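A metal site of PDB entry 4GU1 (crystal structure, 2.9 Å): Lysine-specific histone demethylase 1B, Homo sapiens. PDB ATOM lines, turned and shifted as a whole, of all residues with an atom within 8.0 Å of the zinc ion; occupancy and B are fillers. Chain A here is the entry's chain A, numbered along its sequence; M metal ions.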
ATOM      1  N   GLN A 103     -19.389  30.817   0.122  1.00  0.00           N
ATOM      2  CA  GLN A 103     -18.613  30.454   1.305  1.00  0.00           C
ATOM      3  C   GLN A 103     -17.731  29.225   1.036  1.00  0.00           C
ATOM      4  O   GLN A 103     -18.048  28.388   0.195  1.00  0.00           O
ATOM      5  CB  GLN A 103     -19.536  30.205   2.502  1.00  0.00           C
ATOM      6  CG  GLN A 103     -19.227  31.055   3.729  1.00  0.00           C
ATOM      7  CD  GLN A 103     -20.217  30.799   4.860  1.00  0.00           C
ATOM      8  OE1 GLN A 103     -21.396  30.550   4.620  1.00  0.00           O
ATOM      9  NE2 GLN A 103     -19.726  30.839   6.093  1.00  0.00           N
ATOM     10  N   CYS A 104     -16.604  29.144   1.740  1.00  0.00           N
ATOM     11  CA  CYS A 104     -15.704  28.009   1.598  1.00  0.00           C
ATOM     12  C   CYS A 104     -16.286  26.809   2.313  1.00  0.00           C
ATOM     13  O   CYS A 104     -16.943  26.962   3.339  1.00  0.00           O
ATOM     14  CB  CYS A 104     -14.333  28.361   2.192  1.00  0.00           C
ATOM     15  SG  CYS A 104     -13.011  27.153   1.871  1.00  0.00           S
ATOM     16  N   THR A 105     -16.025  25.623   1.776  1.00  0.00           N
ATOM     17  CA  THR A 105     -16.499  24.364   2.348  1.00  0.00           C
ATOM     18  C   THR A 105     -15.769  23.922   3.615  1.00  0.00           C
ATOM     19  O   THR A 105     -16.418  23.605   4.611  1.00  0.00           O
ATOM     20  CB  THR A 105     -16.421  23.230   1.320  1.00  0.00           C
ATOM     21  OG1 THR A 105     -17.390  23.455   0.286  1.00  0.00           O
ATOM     22  CG2 THR A 105     -16.661  21.858   1.969  1.00  0.00           C
ATOM     23  N   LYS A 106     -14.435  23.901   3.578  1.00  0.00           N
ATOM     24  CA  LYS A 106     -13.652  23.376   4.705  1.00  0.00           C
ATOM     25  C   LYS A 106     -13.896  24.099   6.029  1.00  0.00           C
ATOM     26  O   LYS A 106     -13.887  25.335   6.082  1.00  0.00           O
ATOM     27  CB  LYS A 106     -12.152  23.346   4.388  1.00  0.00           C
ATOM     28  CG  LYS A 106     -11.715  24.139   3.178  1.00  0.00           C
ATOM     29  CD  LYS A 106     -11.029  23.239   2.156  1.00  0.00           C
ATOM     30  CE  LYS A 106     -10.006  23.978   1.301  1.00  0.00           C
ATOM     31  NZ  LYS A 106      -8.685  24.139   1.984  1.00  0.00           N
ATOM     32  N   PRO A 107     -14.087  23.333   7.112  1.00  0.00           N
ATOM     33  CA  PRO A 107     -14.497  23.822   8.448  1.00  0.00           C
ATOM     34  C   PRO A 107     -13.561  24.866   9.035  1.00  0.00           C
ATOM     35  O   PRO A 107     -13.964  25.596   9.948  1.00  0.00           O
ATOM     36  CB  PRO A 107     -14.457  22.561   9.315  1.00  0.00           C
ATOM     37  CG  PRO A 107     -14.552  21.426   8.352  1.00  0.00           C
ATOM     38  CD  PRO A 107     -13.868  21.875   7.114  1.00  0.00           C
ATOM     39  N   GLU A 108     -12.333  24.922   8.522  1.00  0.00           N
ATOM     40  CA  GLU A 108     -11.325  25.851   9.037  1.00  0.00           C
ATOM     41  C   GLU A 108     -11.524  27.251   8.494  1.00  0.00           C
ATOM     42  O   GLU A 108     -11.545  28.232   9.242  1.00  0.00           O
ATOM     43  CB  GLU A 108      -9.926  25.369   8.645  1.00  0.00           C
ATOM     44  CG  GLU A 108      -9.006  25.145   9.818  1.00  0.00           C
ATOM     45  CD  GLU A 108      -9.541  24.086  10.774  1.00  0.00           C
ATOM     46  OE1 GLU A 108      -9.125  24.090  11.948  1.00  0.00           O
ATOM     47  OE2 GLU A 108     -10.359  23.234  10.348  1.00  0.00           O
ATOM     48  N   CYS A 109     -11.685  27.325   7.183  1.00  0.00           N
ATOM     49  CA  CYS A 109     -11.827  28.583   6.468  1.00  0.00           C
ATOM     50  C   CYS A 109     -13.210  29.226   6.693  1.00  0.00           C
ATOM     51  O   CYS A 109     -13.350  30.180   7.478  1.00  0.00           O
ATOM     52  CB  CYS A 109     -11.583  28.335   4.966  1.00  0.00           C
ATOM     53  SG  CYS A 109     -11.118  29.779   3.997  1.00  0.00           S
ATOM     54  N   ARG A 110     -14.216  28.695   5.996  1.00  0.00           N
ATOM     55  CA  ARG A 110     -15.582  29.206   6.017  1.00  0.00           C
ATOM     56  C   ARG A 110     -15.651  30.669   5.567  1.00  0.00           C
ATOM     57  O   ARG A 110     -16.628  31.370   5.832  1.00  0.00           O
ATOM     58  CB  ARG A 110     -16.226  29.018   7.393  1.00  0.00           C
ATOM     59  CG  ARG A 110     -16.058  27.616   7.966  1.00  0.00           C
ATOM     60  CD  ARG A 110     -17.372  26.816   8.009  1.00  0.00           C
ATOM     61  NE  ARG A 110     -18.044  26.755   6.713  1.00  0.00           N
ATOM     62  CZ  ARG A 110     -19.226  27.313   6.457  1.00  0.00           C
ATOM     63  NH1 ARG A 110     -19.874  27.957   7.414  1.00  0.00           N
ATOM     64  NH2 ARG A 110     -19.755  27.214   5.244  1.00  0.00           N
ATOM     65  N   LYS A 111     -14.619  31.122   4.854  1.00  0.00           N
ATOM     66  CA  LYS A 111     -14.526  32.498   4.389  1.00  0.00           C
ATOM     67  C   LYS A 111     -15.451  32.729   3.210  1.00  0.00           C
ATOM     68  O   LYS A 111     -15.702  31.829   2.422  1.00  0.00           O
ATOM     69  CB  LYS A 111     -13.090  32.856   3.995  1.00  0.00           C
ATOM     70  CG  LYS A 111     -12.105  32.896   5.169  1.00  0.00           C
ATOM     71  CD  LYS A 111     -10.755  33.510   4.788  1.00  0.00           C
ATOM     72  CE  LYS A 111      -9.755  33.420   5.936  1.00  0.00           C
ATOM     73  NZ  LYS A 111      -8.468  34.083   5.629  1.00  0.00           N
ATOM     74  N   TRP A 112     -15.955  33.958   3.102  1.00  0.00           N
ATOM     75  CA  TRP A 112     -16.805  34.319   1.975  1.00  0.00           C
ATOM     76  C   TRP A 112     -15.888  34.731   0.834  1.00  0.00           C
ATOM     77  O   TRP A 112     -14.728  35.020   1.065  1.00  0.00           O
ATOM     78  CB  TRP A 112     -17.791  35.431   2.365  1.00  0.00           C
ATOM     79  CG  TRP A 112     -19.030  34.904   3.099  1.00  0.00           C
ATOM     80  CD1 TRP A 112     -19.232  34.830   4.443  1.00  0.00           C
ATOM     81  CD2 TRP A 112     -20.200  34.358   2.493  1.00  0.00           C
ATOM     82  NE1 TRP A 112     -20.451  34.280   4.725  1.00  0.00           N
ATOM     83  CE2 TRP A 112     -21.068  33.973   3.539  1.00  0.00           C
ATOM     84  CE3 TRP A 112     -20.608  34.155   1.175  1.00  0.00           C
ATOM     85  CZ2 TRP A 112     -22.323  33.413   3.303  1.00  0.00           C
ATOM     86  CZ3 TRP A 112     -21.862  33.596   0.940  1.00  0.00           C
ATOM     87  CH2 TRP A 112     -22.693  33.226   1.998  1.00  0.00           C
ATOM     88  N   ARG A 113     -16.390  34.717  -0.396  1.00  0.00           N
ATOM     89  CA  ARG A 113     -15.541  34.965  -1.551  1.00  0.00           C
ATOM     90  C   ARG A 113     -16.304  35.434  -2.784  1.00  0.00           C
ATOM     91  O   ARG A 113     -17.329  34.868  -3.126  1.00  0.00           O
ATOM     92  CB  ARG A 113     -14.759  33.701  -1.912  1.00  0.00           C
ATOM     93  CG  ARG A 113     -13.282  33.930  -2.057  1.00  0.00           C
ATOM     94  CD  ARG A 113     -12.550  33.381  -0.863  1.00  0.00           C
ATOM     95  NE  ARG A 113     -11.616  34.355  -0.288  1.00  0.00           N
ATOM     96  CZ  ARG A 113     -10.754  34.044   0.663  1.00  0.00           C
ATOM     97  NH1 ARG A 113     -10.696  32.793   1.130  1.00  0.00           N
ATOM     98  NH2 ARG A 113      -9.948  34.976   1.154  1.00  0.00           N
ATOM     99  N   TYR A 129     -17.972  24.210  -3.099  1.00  0.00           N
ATOM    100  CA  TYR A 129     -16.914  25.200  -3.360  1.00  0.00           C
ATOM    101  C   TYR A 129     -15.850  25.296  -2.281  1.00  0.00           C
ATOM    102  O   TYR A 129     -16.162  25.370  -1.093  1.00  0.00           O
ATOM    103  CB  TYR A 129     -17.532  26.588  -3.595  1.00  0.00           C
ATOM    104  CG  TYR A 129     -16.538  27.733  -3.696  1.00  0.00           C
ATOM    105  CD1 TYR A 129     -16.102  28.401  -2.551  1.00  0.00           C
ATOM    106  CD2 TYR A 129     -16.065  28.162  -4.930  1.00  0.00           C
ATOM    107  CE1 TYR A 129     -15.189  29.437  -2.646  1.00  0.00           C
ATOM    108  CE2 TYR A 129     -15.170  29.214  -5.029  1.00  0.00           C
ATOM    109  CZ  TYR A 129     -14.729  29.845  -3.881  1.00  0.00           C
ATOM    110  OH  TYR A 129     -13.827  30.883  -3.968  1.00  0.00           O
ATOM    111  N   ARG A 130     -14.593  25.301  -2.708  1.00  0.00           N
ATOM    112  CA  ARG A 130     -13.467  25.641  -1.859  1.00  0.00           C
ATOM    113  C   ARG A 130     -12.683  26.740  -2.578  1.00  0.00           C
ATOM    114  O   ARG A 130     -12.917  26.984  -3.755  1.00  0.00           O
ATOM    115  CB  ARG A 130     -12.609  24.411  -1.555  1.00  0.00           C
ATOM    116  CG  ARG A 130     -13.285  23.441  -0.579  1.00  0.00           C
ATOM    117  CD  ARG A 130     -13.097  21.959  -0.954  1.00  0.00           C
ATOM    118  NE  ARG A 130     -11.830  21.412  -0.463  1.00  0.00           N
ATOM    119  CZ  ARG A 130     -10.725  21.305  -1.198  1.00  0.00           C
ATOM    120  NH1 ARG A 130     -10.713  21.698  -2.465  1.00  0.00           N
ATOM    121  NH2 ARG A 130      -9.621  20.803  -0.661  1.00  0.00           N
ATOM    122  N   CYS A 131     -11.782  27.400  -1.868  1.00  0.00           N
ATOM    123  CA  CYS A 131     -11.065  28.566  -2.426  1.00  0.00           C
ATOM    124  C   CYS A 131     -10.192  28.257  -3.669  1.00  0.00           C
ATOM    125  O   CYS A 131      -9.218  27.507  -3.602  1.00  0.00           O
ATOM    126  CB  CYS A 131     -10.238  29.241  -1.338  1.00  0.00           C
ATOM    127  SG  CYS A 131     -11.201  29.966   0.016  1.00  0.00           S
ATOM    128  N   GLY A 132     -10.551  28.868  -4.800  1.00  0.00           N
ATOM    129  CA  GLY A 132      -9.879  28.585  -6.058  1.00  0.00           C
ATOM    130  C   GLY A 132     -10.532  27.459  -6.834  1.00  0.00           C
ATOM    131  O   GLY A 132     -10.275  26.279  -6.578  1.00  0.00           O
ATOM    132  N   ASP A 145      -1.964  28.071  -1.782  1.00  0.00           N
ATOM    133  CA  ASP A 145      -2.809  28.031  -0.590  1.00  0.00           C
ATOM    134  C   ASP A 145      -3.743  29.253  -0.524  1.00  0.00           C
ATOM    135  O   ASP A 145      -3.428  30.261   0.124  1.00  0.00           O
ATOM    136  CB  ASP A 145      -1.955  27.961   0.680  1.00  0.00           C
ATOM    137  CG  ASP A 145      -2.802  27.863   1.953  1.00  0.00           C
ATOM    138  OD1 ASP A 145      -3.857  27.184   1.917  1.00  0.00           O
ATOM    139  OD2 ASP A 145      -2.404  28.475   2.961  1.00  0.00           O
ATOM    140  N   HIS A 146      -4.886  29.159  -1.204  1.00  0.00           N
ATOM    141  CA  HIS A 146      -5.819  30.271  -1.261  1.00  0.00           C
ATOM    142  C   HIS A 146      -6.476  30.533   0.094  1.00  0.00           C
ATOM    143  O   HIS A 146      -6.836  31.669   0.407  1.00  0.00           O
ATOM    144  CB  HIS A 146      -6.899  30.000  -2.316  1.00  0.00           C
ATOM    145  CG  HIS A 146      -6.359  29.820  -3.704  1.00  0.00           C
ATOM    146  ND1 HIS A 146      -5.498  28.792  -4.040  1.00  0.00           N
ATOM    147  CD2 HIS A 146      -6.574  30.523  -4.847  1.00  0.00           C
ATOM    148  CE1 HIS A 146      -5.210  28.876  -5.327  1.00  0.00           C
ATOM    149  NE2 HIS A 146      -5.846  29.914  -5.844  1.00  0.00           N
ATOM    150  N   CYS A 147      -6.591  29.481   0.913  1.00  0.00           N
ATOM    151  CA  CYS A 147      -7.326  29.523   2.179  1.00  0.00           C
ATOM    152  C   CYS A 147      -6.705  30.400   3.274  1.00  0.00           C
ATOM    153  O   CYS A 147      -7.126  30.348   4.433  1.00  0.00           O
ATOM    154  CB  CYS A 147      -7.539  28.105   2.729  1.00  0.00           C
ATOM    155  SG  CYS A 147      -9.133  27.307   2.328  1.00  0.00           S
ATOM    156  N   SER A 148      -5.719  31.204   2.912  1.00  0.00           N
ATOM    157  CA  SER A 148      -5.105  32.127   3.854  1.00  0.00           C
ATOM    158  C   SER A 148      -5.277  33.570   3.376  1.00  0.00           C
ATOM    159  O   SER A 148      -5.134  34.513   4.163  1.00  0.00           O
ATOM    160  CB  SER A 148      -3.630  31.788   4.071  1.00  0.00           C
ATOM    161  OG  SER A 148      -2.908  31.781   2.851  1.00  0.00           O
ATOM    162  N   LEU A 149      -5.603  33.738   2.087  1.00  0.00           N
ATOM    163  CA  LEU A 149      -5.876  35.059   1.517  1.00  0.00           C
ATOM    164  C   LEU A 149      -6.903  35.791   2.372  1.00  0.00           C
ATOM    165  O   LEU A 149      -7.907  35.199   2.787  1.00  0.00           O
ATOM    166  CB  LEU A 149      -6.371  34.956   0.072  1.00  0.00           C
ATOM    167  CG  LEU A 149      -5.317  34.982  -1.047  1.00  0.00           C
ATOM    168  CD1 LEU A 149      -4.409  33.762  -0.968  1.00  0.00           C
ATOM    169  CD2 LEU A 149      -5.974  35.093  -2.417  1.00  0.00           C
HETATM  170 ZN    ZN M   1     -11.130  28.580   1.989  1.00  0.00          ZN
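The guanidinium group (NH2) of Arg 110 lies within hydrogen-bond range of the backbone carbonyl oxygen (O) of Cys 104, at 3.4 Å.
The side-chain sulfur of Cys 147 lies close to the side-chain amino group of Lys 106.
The side-chain sulfur of Cys 131 sits close to the guanidinium group of Arg 113 (3.1 Å).
N of Cys 104 is in hydrogen-bond range of O of Lys 111, at 2.9 Å.
Of the 20 residues printed, 4 come within 4 Å of the zinc ion.
The nearest printed residue that does not touch the zinc ion is Arg 113 (4.3 Å).
The zinc ion is bound by the side-chain sulfur (SG) of Cys 109 (2.3 Å), the side-chain sulfur (SG) of Cys 104 (2.4 Å), the side-chain sulfur (SG) of Cys 147 (2.4 Å) and the side-chain sulfur (SG) of Cys 131 (2.4 Å).
The zinc ion has four donor atoms within binding distance.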
